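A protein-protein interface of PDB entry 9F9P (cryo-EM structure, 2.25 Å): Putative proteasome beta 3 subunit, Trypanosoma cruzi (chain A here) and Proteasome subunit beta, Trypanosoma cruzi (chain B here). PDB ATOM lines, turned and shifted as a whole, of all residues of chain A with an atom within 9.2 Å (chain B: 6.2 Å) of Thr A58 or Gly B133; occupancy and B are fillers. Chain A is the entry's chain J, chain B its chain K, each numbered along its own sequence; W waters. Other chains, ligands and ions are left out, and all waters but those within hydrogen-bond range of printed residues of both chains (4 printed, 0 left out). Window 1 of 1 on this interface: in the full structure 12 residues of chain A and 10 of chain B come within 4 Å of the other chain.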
ATOM      1  N   ILE A   3     -26.565   0.873  12.660  1.00  0.00           N
ATOM      2  CA  ILE A   3     -26.755   0.857  11.218  1.00  0.00           C
ATOM      3  C   ILE A   3     -27.897   1.809  10.825  1.00  0.00           C
ATOM      4  O   ILE A   3     -27.844   2.432   9.777  1.00  0.00           O
ATOM      5  CB  ILE A   3     -26.996  -0.582  10.706  1.00  0.00           C
ATOM      6  CG1 ILE A   3     -25.822  -1.515  11.005  1.00  0.00           C
ATOM      7  CG2 ILE A   3     -27.296  -0.616   9.222  1.00  0.00           C
ATOM      8  CD1 ILE A   3     -26.179  -2.997  10.907  1.00  0.00           C
ATOM      9  N   TYR A   6     -26.491   5.503  10.593  1.00  0.00           N
ATOM     10  CA  TYR A   6     -25.325   5.792   9.775  1.00  0.00           C
ATOM     11  C   TYR A   6     -25.584   6.928   8.778  1.00  0.00           C
ATOM     12  O   TYR A   6     -24.744   7.815   8.620  1.00  0.00           O
ATOM     13  CB  TYR A   6     -24.850   4.477   9.155  1.00  0.00           C
ATOM     14  CG  TYR A   6     -23.605   4.557   8.315  1.00  0.00           C
ATOM     15  CD1 TYR A   6     -22.343   4.481   8.882  1.00  0.00           C
ATOM     16  CD2 TYR A   6     -23.698   4.752   6.941  1.00  0.00           C
ATOM     17  CE1 TYR A   6     -21.203   4.549   8.093  1.00  0.00           C
ATOM     18  CE2 TYR A   6     -22.571   4.847   6.138  1.00  0.00           C
ATOM     19  CZ  TYR A   6     -21.320   4.724   6.713  1.00  0.00           C
ATOM     20  OH  TYR A   6     -20.214   4.836   5.901  1.00  0.00           O
ATOM     21  N   SER A   7     -26.753   6.983   8.142  1.00  0.00           N
ATOM     22  CA  SER A   7     -26.915   7.845   6.977  1.00  0.00           C
ATOM     23  C   SER A   7     -27.554   9.187   7.295  1.00  0.00           C
ATOM     24  O   SER A   7     -27.514  10.083   6.459  1.00  0.00           O
ATOM     25  CB  SER A   7     -27.714   7.146   5.882  1.00  0.00           C
ATOM     26  OG  SER A   7     -26.879   6.259   5.107  1.00  0.00           O
ATOM     27  N   LEU A  28     -27.688  14.143   3.953  1.00  0.00           N
ATOM     28  CA  LEU A  28     -27.159  12.802   3.734  1.00  0.00           C
ATOM     29  C   LEU A  28     -25.718  12.716   4.226  1.00  0.00           C
ATOM     30  O   LEU A  28     -24.883  13.491   3.782  1.00  0.00           O
ATOM     31  CB  LEU A  28     -27.212  12.468   2.243  1.00  0.00           C
ATOM     32  CG  LEU A  28     -26.468  11.188   1.860  1.00  0.00           C
ATOM     33  CD1 LEU A  28     -27.159   9.942   2.409  1.00  0.00           C
ATOM     34  CD2 LEU A  28     -26.364  11.040   0.364  1.00  0.00           C
ATOM     35  N   GLY A  29     -25.441  11.753   5.104  1.00  0.00           N
ATOM     36  CA  GLY A  29     -24.112  11.654   5.654  1.00  0.00           C
ATOM     37  C   GLY A  29     -23.493  10.263   5.720  1.00  0.00           C
ATOM     38  O   GLY A  29     -24.077   9.271   5.324  1.00  0.00           O
ATOM     39  N   GLU A  30     -22.258  10.236   6.220  1.00  0.00           N
ATOM     40  CA  GLU A  30     -21.579   9.032   6.668  1.00  0.00           C
ATOM     41  C   GLU A  30     -21.125   9.232   8.109  1.00  0.00           C
ATOM     42  O   GLU A  30     -20.034   9.753   8.309  1.00  0.00           O
ATOM     43  CB  GLU A  30     -20.364   8.757   5.769  1.00  0.00           C
ATOM     44  CG  GLU A  30     -20.688   8.175   4.405  1.00  0.00           C
ATOM     45  CD  GLU A  30     -19.603   8.181   3.309  1.00  0.00           C
ATOM     46  OE1 GLU A  30     -19.932   7.783   2.132  1.00  0.00           O
ATOM     47  OE2 GLU A  30     -18.418   8.583   3.601  1.00  0.00           O
ATOM     48  N   LEU A  53     -39.149   7.434   3.812  1.00  0.00           N
ATOM     49  CA  LEU A  53     -38.284   6.338   4.198  1.00  0.00           C
ATOM     50  C   LEU A  53     -37.043   6.866   4.893  1.00  0.00           C
ATOM     51  O   LEU A  53     -36.306   7.641   4.305  1.00  0.00           O
ATOM     52  CB  LEU A  53     -37.795   5.584   2.968  1.00  0.00           C
ATOM     53  CG  LEU A  53     -38.707   4.531   2.364  1.00  0.00           C
ATOM     54  CD1 LEU A  53     -38.055   3.947   1.124  1.00  0.00           C
ATOM     55  CD2 LEU A  53     -38.992   3.403   3.348  1.00  0.00           C
ATOM     56  N   THR A  54     -36.741   6.300   6.056  1.00  0.00           N
ATOM     57  CA  THR A  54     -35.533   6.607   6.791  1.00  0.00           C
ATOM     58  C   THR A  54     -34.788   5.314   7.043  1.00  0.00           C
ATOM     59  O   THR A  54     -35.355   4.267   6.813  1.00  0.00           O
ATOM     60  CB  THR A  54     -35.876   7.271   8.129  1.00  0.00           C
ATOM     61  OG1 THR A  54     -36.627   6.369   8.955  1.00  0.00           O
ATOM     62  CG2 THR A  54     -36.652   8.552   7.897  1.00  0.00           C
ATOM     63  N   GLY A  55     -33.562   5.409   7.532  1.00  0.00           N
ATOM     64  CA  GLY A  55     -32.690   4.262   7.722  1.00  0.00           C
ATOM     65  C   GLY A  55     -31.435   4.371   6.861  1.00  0.00           C
ATOM     66  O   GLY A  55     -31.081   5.454   6.420  1.00  0.00           O
ATOM     67  N   LEU A  56     -30.796   3.234   6.586  1.00  0.00           N
ATOM     68  CA  LEU A  56     -29.584   3.200   5.795  1.00  0.00           C
ATOM     69  C   LEU A  56     -29.866   3.611   4.345  1.00  0.00           C
ATOM     70  O   LEU A  56     -30.813   3.167   3.744  1.00  0.00           O
ATOM     71  CB  LEU A  56     -29.069   1.777   5.915  1.00  0.00           C
ATOM     72  CG  LEU A  56     -27.698   1.515   5.292  1.00  0.00           C
ATOM     73  CD1 LEU A  56     -26.569   2.199   6.065  1.00  0.00           C
ATOM     74  CD2 LEU A  56     -27.429   0.027   5.249  1.00  0.00           C
ATOM     75  N   ARG A  57     -29.059   4.445   3.734  1.00  0.00           N
ATOM     76  CA  ARG A  57     -29.472   5.029   2.463  1.00  0.00           C
ATOM     77  C   ARG A  57     -29.505   4.012   1.310  1.00  0.00           C
ATOM     78  O   ARG A  57     -30.387   4.112   0.466  1.00  0.00           O
ATOM     79  CB  ARG A  57     -28.607   6.240   2.114  1.00  0.00           C
ATOM     80  CG  ARG A  57     -28.879   6.903   0.766  1.00  0.00           C
ATOM     81  CD  ARG A  57     -30.178   7.673   0.738  1.00  0.00           C
ATOM     82  NE  ARG A  57     -30.410   8.339  -0.523  1.00  0.00           N
ATOM     83  CZ  ARG A  57     -31.604   8.786  -0.918  1.00  0.00           C
ATOM     84  NH1 ARG A  57     -32.685   8.627  -0.178  1.00  0.00           N
ATOM     85  NH2 ARG A  57     -31.754   9.399  -2.072  1.00  0.00           N
ATOM     86  N   THR A  58     -28.589   3.052   1.252  1.00  0.00           N
ATOM     87  CA  THR A  58     -28.610   2.003   0.239  1.00  0.00           C
ATOM     88  C   THR A  58     -29.904   1.190   0.281  1.00  0.00           C
ATOM     89  O   THR A  58     -30.491   0.951  -0.758  1.00  0.00           O
ATOM     90  CB  THR A  58     -27.376   1.117   0.344  1.00  0.00           C
ATOM     91  OG1 THR A  58     -27.362   0.181  -0.729  1.00  0.00           O
ATOM     92  CG2 THR A  58     -27.317   0.338   1.640  1.00  0.00           C
ATOM     93  N   ASP A  59     -30.421   0.865   1.486  1.00  0.00           N
ATOM     94  CA  ASP A  59     -31.709   0.200   1.641  1.00  0.00           C
ATOM     95  C   ASP A  59     -32.897   1.141   1.390  1.00  0.00           C
ATOM     96  O   ASP A  59     -33.872   0.726   0.795  1.00  0.00           O
ATOM     97  CB  ASP A  59     -31.783  -0.472   3.002  1.00  0.00           C
ATOM     98  CG  ASP A  59     -30.882  -1.695   3.170  1.00  0.00           C
ATOM     99  OD1 ASP A  59     -30.183  -2.133   2.157  1.00  0.00           O
ATOM    100  OD2 ASP A  59     -30.872  -2.264   4.310  1.00  0.00           O
ATOM    101  N   GLN A  60     -32.844   2.421   1.707  1.00  0.00           N
ATOM    102  CA  GLN A  60     -33.877   3.295   1.189  1.00  0.00           C
ATOM    103  C   GLN A  60     -33.927   3.274  -0.348  1.00  0.00           C
ATOM    104  O   GLN A  60     -35.003   3.311  -0.924  1.00  0.00           O
ATOM    105  CB  GLN A  60     -33.718   4.780   1.522  1.00  0.00           C
ATOM    106  CG  GLN A  60     -33.652   5.148   3.007  1.00  0.00           C
ATOM    107  CD  GLN A  60     -33.269   6.607   3.232  1.00  0.00           C
ATOM    108  OE1 GLN A  60     -33.639   7.508   2.475  1.00  0.00           O
ATOM    109  NE2 GLN A  60     -32.434   6.866   4.228  1.00  0.00           N
ATOM    110  N   GLN A  61     -32.803   3.310  -1.058  1.00  0.00           N
ATOM    111  CA  GLN A  61     -32.855   3.383  -2.508  1.00  0.00           C
ATOM    112  C   GLN A  61     -33.327   2.045  -3.080  1.00  0.00           C
ATOM    113  O   GLN A  61     -34.150   2.036  -3.966  1.00  0.00           O
ATOM    114  CB  GLN A  61     -31.468   3.768  -3.073  1.00  0.00           C
ATOM    115  CG  GLN A  61     -31.029   5.200  -2.720  1.00  0.00           C
ATOM    116  CD  GLN A  61     -29.685   5.606  -3.259  1.00  0.00           C
ATOM    117  OE1 GLN A  61     -28.637   5.192  -2.804  1.00  0.00           O
ATOM    118  NE2 GLN A  61     -29.687   6.453  -4.258  1.00  0.00           N
ATOM    119  N   THR A  62     -32.835   0.911  -2.558  1.00  0.00           N
ATOM    120  CA  THR A  62     -33.225  -0.420  -3.013  1.00  0.00           C
ATOM    121  C   THR A  62     -34.697  -0.710  -2.706  1.00  0.00           C
ATOM    122  O   THR A  62     -35.462  -1.131  -3.561  1.00  0.00           O
ATOM    123  CB  THR A  62     -32.301  -1.492  -2.417  1.00  0.00           C
ATOM    124  OG1 THR A  62     -30.934  -1.364  -2.837  1.00  0.00           O
ATOM    125  CG2 THR A  62     -32.714  -2.885  -2.833  1.00  0.00           C
ATOM    126  N   PHE A  63     -35.148  -0.391  -1.506  1.00  0.00           N
ATOM    127  CA  PHE A  63     -36.509  -0.719  -1.139  1.00  0.00           C
ATOM    128  C   PHE A  63     -37.519   0.155  -1.875  1.00  0.00           C
ATOM    129  O   PHE A  63     -38.568  -0.328  -2.285  1.00  0.00           O
ATOM    130  CB  PHE A  63     -36.670  -0.705   0.378  1.00  0.00           C
ATOM    131  CG  PHE A  63     -38.023  -1.131   0.846  1.00  0.00           C
ATOM    132  CD1 PHE A  63     -38.302  -2.466   1.053  1.00  0.00           C
ATOM    133  CD2 PHE A  63     -38.999  -0.202   1.079  1.00  0.00           C
ATOM    134  CE1 PHE A  63     -39.553  -2.864   1.492  1.00  0.00           C
ATOM    135  CE2 PHE A  63     -40.269  -0.580   1.501  1.00  0.00           C
ATOM    136  CZ  PHE A  63     -40.546  -1.913   1.659  1.00  0.00           C
ATOM    137  N   SER A  64     -37.217   1.413  -2.104  1.00  0.00           N
ATOM    138  CA  SER A  64     -38.156   2.224  -2.833  1.00  0.00           C
ATOM    139  C   SER A  64     -38.238   1.827  -4.303  1.00  0.00           C
ATOM    140  O   SER A  64     -39.287   1.944  -4.884  1.00  0.00           O
ATOM    141  CB  SER A  64     -37.879   3.693  -2.682  1.00  0.00           C
ATOM    142  OG  SER A  64     -36.609   4.052  -3.216  1.00  0.00           O
ATOM    143  N   GLU A  65     -37.153   1.400  -4.935  1.00  0.00           N
ATOM    144  CA  GLU A  65     -37.221   0.869  -6.295  1.00  0.00           C
ATOM    145  C   GLU A  65     -38.074  -0.402  -6.391  1.00  0.00           C
ATOM    146  O   GLU A  65     -38.822  -0.525  -7.335  1.00  0.00           O
ATOM    147  CB  GLU A  65     -35.822   0.579  -6.842  1.00  0.00           C
ATOM    148  CG  GLU A  65     -35.070   1.850  -7.199  1.00  0.00           C
ATOM    149  CD  GLU A  65     -33.544   1.788  -7.309  1.00  0.00           C
ATOM    150  OE1 GLU A  65     -32.974   0.652  -7.380  1.00  0.00           O
ATOM    151  OE2 GLU A  65     -32.898   2.893  -7.307  1.00  0.00           O
ATOM    152  N   LYS A  66     -37.950  -1.346  -5.447  1.00  0.00           N
ATOM    153  CA  LYS A  66     -38.807  -2.514  -5.441  1.00  0.00           C
ATOM    154  C   LYS A  66     -40.274  -2.160  -5.294  1.00  0.00           C
ATOM    155  O   LYS A  66     -41.116  -2.845  -5.852  1.00  0.00           O
ATOM    156  CB  LYS A  66     -38.477  -3.501  -4.336  1.00  0.00           C
ATOM    157  CG  LYS A  66     -37.116  -4.142  -4.489  1.00  0.00           C
ATOM    158  CD  LYS A  66     -36.864  -5.282  -3.514  1.00  0.00           C
ATOM    159  CE  LYS A  66     -35.413  -5.753  -3.597  1.00  0.00           C
ATOM    160  NZ  LYS A  66     -35.034  -6.355  -4.910  1.00  0.00           N
ATOM    161  N   TRP A 103     -34.380  -5.474   5.778  1.00  0.00           N
ATOM    162  CA  TRP A 103     -34.090  -4.181   5.181  1.00  0.00           C
ATOM    163  C   TRP A 103     -33.946  -3.145   6.288  1.00  0.00           C
ATOM    164  O   TRP A 103     -34.888  -2.980   7.055  1.00  0.00           O
ATOM    165  CB  TRP A 103     -35.231  -3.782   4.224  1.00  0.00           C
ATOM    166  CG  TRP A 103     -35.395  -4.689   3.042  1.00  0.00           C
ATOM    167  CD1 TRP A 103     -36.401  -5.575   2.814  1.00  0.00           C
ATOM    168  CD2 TRP A 103     -34.507  -4.815   1.940  1.00  0.00           C
ATOM    169  NE1 TRP A 103     -36.182  -6.286   1.675  1.00  0.00           N
ATOM    170  CE2 TRP A 103     -35.041  -5.821   1.095  1.00  0.00           C
ATOM    171  CE3 TRP A 103     -33.316  -4.169   1.574  1.00  0.00           C
ATOM    172  CZ2 TRP A 103     -34.433  -6.188  -0.105  1.00  0.00           C
ATOM    173  CZ3 TRP A 103     -32.679  -4.570   0.411  1.00  0.00           C
ATOM    174  CH2 TRP A 103     -33.233  -5.573  -0.411  1.00  0.00           C
ATOM    175  N   PHE A 104     -32.856  -2.376   6.343  1.00  0.00           N
ATOM    176  CA  PHE A 104     -32.724  -1.400   7.441  1.00  0.00           C
ATOM    177  C   PHE A 104     -33.400  -0.074   7.117  1.00  0.00           C
ATOM    178  O   PHE A 104     -32.722   0.877   6.842  1.00  0.00           O
ATOM    179  CB  PHE A 104     -31.250  -1.170   7.770  1.00  0.00           C
ATOM    180  CG  PHE A 104     -30.601  -2.392   8.339  1.00  0.00           C
ATOM    181  CD1 PHE A 104     -30.814  -2.743   9.661  1.00  0.00           C
ATOM    182  CD2 PHE A 104     -29.840  -3.226   7.536  1.00  0.00           C
ATOM    183  CE1 PHE A 104     -30.313  -3.938  10.171  1.00  0.00           C
ATOM    184  CE2 PHE A 104     -29.295  -4.400   8.051  1.00  0.00           C
ATOM    185  CZ  PHE A 104     -29.539  -4.758   9.369  1.00  0.00           C
ATOM    186  N   VAL A 105     -34.731  -0.060   7.076  1.00  0.00           N
ATOM    187  CA  VAL A 105     -35.541   1.106   6.748  1.00  0.00           C
ATOM    188  C   VAL A 105     -36.707   1.169   7.704  1.00  0.00           C
ATOM    189  O   VAL A 105     -37.148   0.146   8.186  1.00  0.00           O
ATOM    190  CB  VAL A 105     -36.138   1.057   5.328  1.00  0.00           C
ATOM    191  CG1 VAL A 105     -35.090   1.106   4.272  1.00  0.00           C
ATOM    192  CG2 VAL A 105     -36.979  -0.174   5.095  1.00  0.00           C
ATOM    193  N   ARG B  87     -24.929   0.760  -9.107  1.00  0.00           N
ATOM    194  CA  ARG B  87     -25.462   0.816  -7.757  1.00  0.00           C
ATOM    195  C   ARG B  87     -26.161  -0.492  -7.403  1.00  0.00           C
ATOM    196  O   ARG B  87     -26.010  -1.047  -6.332  1.00  0.00           O
ATOM    197  CB  ARG B  87     -26.480   1.968  -7.640  1.00  0.00           C
ATOM    198  CG  ARG B  87     -26.789   2.318  -6.195  1.00  0.00           C
ATOM    199  CD  ARG B  87     -28.177   2.842  -5.922  1.00  0.00           C
ATOM    200  NE  ARG B  87     -29.179   1.828  -5.921  1.00  0.00           N
ATOM    201  CZ  ARG B  87     -29.427   1.035  -4.914  1.00  0.00           C
ATOM    202  NH1 ARG B  87     -30.408   0.174  -5.049  1.00  0.00           N
ATOM    203  NH2 ARG B  87     -28.750   1.093  -3.782  1.00  0.00           N
ATOM    204  N   LEU B  90     -23.475  -3.098  -6.770  1.00  0.00           N
ATOM    205  CA  LEU B  90     -22.909  -2.970  -5.426  1.00  0.00           C
ATOM    206  C   LEU B  90     -23.867  -3.420  -4.321  1.00  0.00           C
ATOM    207  O   LEU B  90     -23.484  -4.185  -3.454  1.00  0.00           O
ATOM    208  CB  LEU B  90     -22.480  -1.533  -5.182  1.00  0.00           C
ATOM    209  CG  LEU B  90     -21.326  -1.044  -6.037  1.00  0.00           C
ATOM    210  CD1 LEU B  90     -21.297   0.474  -6.047  1.00  0.00           C
ATOM    211  CD2 LEU B  90     -20.006  -1.595  -5.541  1.00  0.00           C
ATOM    212  N   ALA B  91     -25.104  -2.941  -4.337  1.00  0.00           N
ATOM    213  CA  ALA B  91     -26.129  -3.358  -3.371  1.00  0.00           C
ATOM    214  C   ALA B  91     -26.443  -4.855  -3.427  1.00  0.00           C
ATOM    215  O   ALA B  91     -26.640  -5.473  -2.389  1.00  0.00           O
ATOM    216  CB  ALA B  91     -27.378  -2.588  -3.611  1.00  0.00           C
ATOM    217  N   LEU B  94     -23.724  -6.870  -1.585  1.00  0.00           N
ATOM    218  CA  LEU B  94     -23.740  -6.681  -0.143  1.00  0.00           C
ATOM    219  C   LEU B  94     -24.558  -7.766   0.561  1.00  0.00           C
ATOM    220  O   LEU B  94     -24.182  -8.214   1.641  1.00  0.00           O
ATOM    221  CB  LEU B  94     -24.306  -5.276   0.143  1.00  0.00           C
ATOM    222  CG  LEU B  94     -24.488  -4.901   1.608  1.00  0.00           C
ATOM    223  CD1 LEU B  94     -23.139  -4.552   2.231  1.00  0.00           C
ATOM    224  CD2 LEU B  94     -25.461  -3.721   1.733  1.00  0.00           C
ATOM    225  N   ARG B  95     -25.643  -8.213  -0.079  1.00  0.00           N
ATOM    226  CA  ARG B  95     -26.496  -9.243   0.501  1.00  0.00           C
ATOM    227  C   ARG B  95     -26.235 -10.623  -0.106  1.00  0.00           C
ATOM    228  O   ARG B  95     -27.006 -11.546   0.124  1.00  0.00           O
ATOM    229  CB  ARG B  95     -27.969  -8.827   0.379  1.00  0.00           C
ATOM    230  CG  ARG B  95     -28.375  -7.800   1.429  1.00  0.00           C
ATOM    231  CD  ARG B  95     -29.865  -7.623   1.647  1.00  0.00           C
ATOM    232  NE  ARG B  95     -30.152  -6.826   2.845  1.00  0.00           N
ATOM    233  CZ  ARG B  95     -29.927  -5.519   2.944  1.00  0.00           C
ATOM    234  NH1 ARG B  95     -29.399  -4.847   1.927  1.00  0.00           N
ATOM    235  NH2 ARG B  95     -30.237  -4.877   4.054  1.00  0.00           N
ATOM    236  N   MET B 129     -20.550   7.316  -5.328  1.00  0.00           N
ATOM    237  CA  MET B 129     -21.059   6.055  -4.805  1.00  0.00           C
ATOM    238  C   MET B 129     -20.180   5.520  -3.700  1.00  0.00           C
ATOM    239  O   MET B 129     -18.993   5.773  -3.715  1.00  0.00           O
ATOM    240  CB  MET B 129     -21.044   4.941  -5.831  1.00  0.00           C
ATOM    241  CG  MET B 129     -21.403   5.412  -7.176  1.00  0.00           C
ATOM    242  SD  MET B 129     -22.287   4.148  -8.126  1.00  0.00           S
ATOM    243  CE  MET B 129     -22.171   5.046  -9.665  1.00  0.00           C
ATOM    244  N   ASP B 130     -20.738   4.691  -2.817  1.00  0.00           N
ATOM    245  CA  ASP B 130     -19.911   3.986  -1.850  1.00  0.00           C
ATOM    246  C   ASP B 130     -20.071   2.471  -1.973  1.00  0.00           C
ATOM    247  O   ASP B 130     -20.939   1.969  -2.654  1.00  0.00           O
ATOM    248  CB  ASP B 130     -20.170   4.530  -0.459  1.00  0.00           C
ATOM    249  CG  ASP B 130     -21.389   3.999   0.276  1.00  0.00           C
ATOM    250  OD1 ASP B 130     -22.067   3.077  -0.243  1.00  0.00           O
ATOM    251  OD2 ASP B 130     -21.686   4.539   1.406  1.00  0.00           O
ATOM    252  N   TYR B 131     -19.248   1.730  -1.249  1.00  0.00           N
ATOM    253  CA  TYR B 131     -19.212   0.285  -1.371  1.00  0.00           C
ATOM    254  C   TYR B 131     -20.522  -0.400  -0.987  1.00  0.00           C
ATOM    255  O   TYR B 131     -20.709  -1.553  -1.343  1.00  0.00           O
ATOM    256  CB  TYR B 131     -18.038  -0.258  -0.549  1.00  0.00           C
ATOM    257  CG  TYR B 131     -18.227  -0.294   0.936  1.00  0.00           C
ATOM    258  CD1 TYR B 131     -18.096   0.854   1.723  1.00  0.00           C
ATOM    259  CD2 TYR B 131     -18.591  -1.484   1.551  1.00  0.00           C
ATOM    260  CE1 TYR B 131     -18.297   0.805   3.103  1.00  0.00           C
ATOM    261  CE2 TYR B 131     -18.777  -1.552   2.929  1.00  0.00           C
ATOM    262  CZ  TYR B 131     -18.624  -0.410   3.706  1.00  0.00           C
ATOM    263  OH  TYR B 131     -18.856  -0.540   5.062  1.00  0.00           O
ATOM    264  N   LEU B 132     -21.399   0.255  -0.222  1.00  0.00           N
ATOM    265  CA  LEU B 132     -22.675  -0.306   0.207  1.00  0.00           C
ATOM    266  C   LEU B 132     -23.737  -0.200  -0.887  1.00  0.00           C
ATOM    267  O   LEU B 132     -24.772  -0.859  -0.817  1.00  0.00           O
ATOM    268  CB  LEU B 132     -23.172   0.478   1.434  1.00  0.00           C
ATOM    269  CG  LEU B 132     -22.361   0.332   2.735  1.00  0.00           C
ATOM    270  CD1 LEU B 132     -22.813   1.310   3.811  1.00  0.00           C
ATOM    271  CD2 LEU B 132     -22.453  -1.061   3.322  1.00  0.00           C
ATOM    272  N   GLY B 133     -23.540   0.687  -1.859  1.00  0.00           N
ATOM    273  CA  GLY B 133     -24.571   0.963  -2.852  1.00  0.00           C
ATOM    274  C   GLY B 133     -25.320   2.277  -2.662  1.00  0.00           C
ATOM    275  O   GLY B 133     -26.401   2.463  -3.207  1.00  0.00           O
ATOM    276  N   THR B 134     -24.752   3.213  -1.916  1.00  0.00           N
ATOM    277  CA  THR B 134     -25.340   4.540  -1.832  1.00  0.00           C
ATOM    278  C   THR B 134     -25.007   5.318  -3.106  1.00  0.00           C
ATOM    279  O   THR B 134     -23.874   5.263  -3.530  1.00  0.00           O
ATOM    280  CB  THR B 134     -24.705   5.235  -0.630  1.00  0.00           C
ATOM    281  OG1 THR B 134     -24.784   4.400   0.524  1.00  0.00           O
ATOM    282  CG2 THR B 134     -25.337   6.569  -0.332  1.00  0.00           C
ATOM    283  N   MET B 135     -25.892   6.107  -3.686  1.00  0.00           N
ATOM    284  CA  MET B 135     -25.561   6.805  -4.919  1.00  0.00           C
ATOM    285  C   MET B 135     -26.251   8.166  -4.949  1.00  0.00           C
ATOM    286  O   MET B 135     -27.422   8.259  -4.637  1.00  0.00           O
ATOM    287  CB  MET B 135     -26.048   6.017  -6.124  1.00  0.00           C
ATOM    288  CG  MET B 135     -25.958   6.774  -7.447  1.00  0.00           C
ATOM    289  SD  MET B 135     -26.913   5.928  -8.769  1.00  0.00           S
ATOM    290  CE  MET B 135     -28.333   6.974  -9.067  1.00  0.00           C
HETATM  291  O   HOH W   1     -28.537   9.498  -2.455  1.00  0.00           O
HETATM  292  O   HOH W   2     -19.979   4.295   3.269  1.00  0.00           O
HETATM  293  O   HOH W   3     -33.147  -7.505   3.346  1.00  0.00           O
HETATM  294  O   HOH W   4     -30.432   1.592  -8.877  1.00  0.00           O
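Printed residues of chain B within 4 Å of Arg A57: Thr B134 (3.7 Å).
Of the printed residues of chain B, Thr A58 touches Arg B87, Ala B91, Leu B132 and Gly B133.
Of the printed residues of chain B, Trp A103 touches Arg B95.
Printed residues of chain A within 4 Å of Arg B87: Thr A58, Gln A61, Thr A62 and Glu A65.
Of the printed residues of chain A, Ala B91 touches Thr A58 (3.997 Å) and Thr A62 (3.8 Å).
Thr B134 touches two residues of chain A.
Asp B130 touches Glu A30.
CG of Arg A57 touches CG2 of Thr B134, at 3.7 Å.
OG1 of Thr A58 touches CB of Ala B91, at 3.997 Å.
Gly B133 touches Thr A58.
CZ of Arg B87 touches CB of Gln A61, 3.9 Å away.
Gln A61 touches Gly B133.
OE1 of Gln A61 touches CA of Thr B134, at 3.5 Å.
Thr A62 touches Ala B91 (OG1 to CB, 3.8 Å).
Trp A103 touches Arg B95.
Phe A104 touches Arg B95.
OE1 of Gln A60 is in hydrogen-bond range of NH1 of Arg A57 (3.0 Å).
OG of Ser A64 sits at hydrogen-bond distance from O of Gln A61 (3.3 Å).
NH2 of Arg B87 sits at hydrogen-bond distance from O of Gly B133.
The side-chain carboxylate (OD1) of Asp B130 sits at hydrogen-bond distance from the backbone NH (N) of Leu B132 (2.9 Å).
The backbone carbonyl oxygen (O) of Thr A58 lies within hydrogen-bond range of the side-chain hydroxyl (OG1) of Thr A62, 3.1 Å away.
OD1 of Asp B130 sits at hydrogen-bond distance from OG1 of Thr B134 (3.1 Å).
Of the 12 printed residues of chain B, 8 touch a printed residue of chain A.
Hydrophobic or aromatic side chains of chain B within 4 Å of the printed part of chain A: Ala B91.
Of the 23 printed residues of chain A, 9 touch a printed residue of chain B.
Among the printed residues, Asp or Glu carboxylates within 4 Å of a Lys or Arg side-chain nitrogen of the other chain: Asp A59 with Arg B95 and Glu A65 with Arg B87.
The side-chain amide nitrogen (NE2) of Gln A61 lies within hydrogen-bond range of the backbone carbonyl oxygen (O) of Met B135 (2.9 Å).
OG1 of Thr A58 is in hydrogen-bond range of O of Leu B132 (2.8 Å).
The guanidinium group of Arg B87 sits at hydrogen-bond distance from the side-chain hydroxyl of Thr A58 (3.5 Å).
The side-chain carboxylate of Glu A65 lies within salt-bridge range of the guanidinium group of Arg B87, 3.5 Å away.
The guanidinium group (NH2) of Arg B95 lies within salt-bridge range of the side-chain carboxylate (OD2) of Asp A59, at 2.7 Å.
OG1 of Thr A62 is in hydrogen-bond range of NH1 of Arg B87 (2.7 Å).
Water W2 lies within hydrogen-bond range of OD2 of Asp B130 (2.5 Å) and OH of Tyr A6 (2.7 Å).
Water W1 bridges O of Met B135 and NE of Arg A57.
Water W4 lies within hydrogen-bond range of the side-chain carboxylate of Glu A65 (3.1 Å) and the guanidinium group of Arg B87 (3.2 Å).
Water W3 lies within hydrogen-bond range of the guanidinium group of Arg B95 (3.1 Å) and the backbone NH of Trp A103 (3.4 Å).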
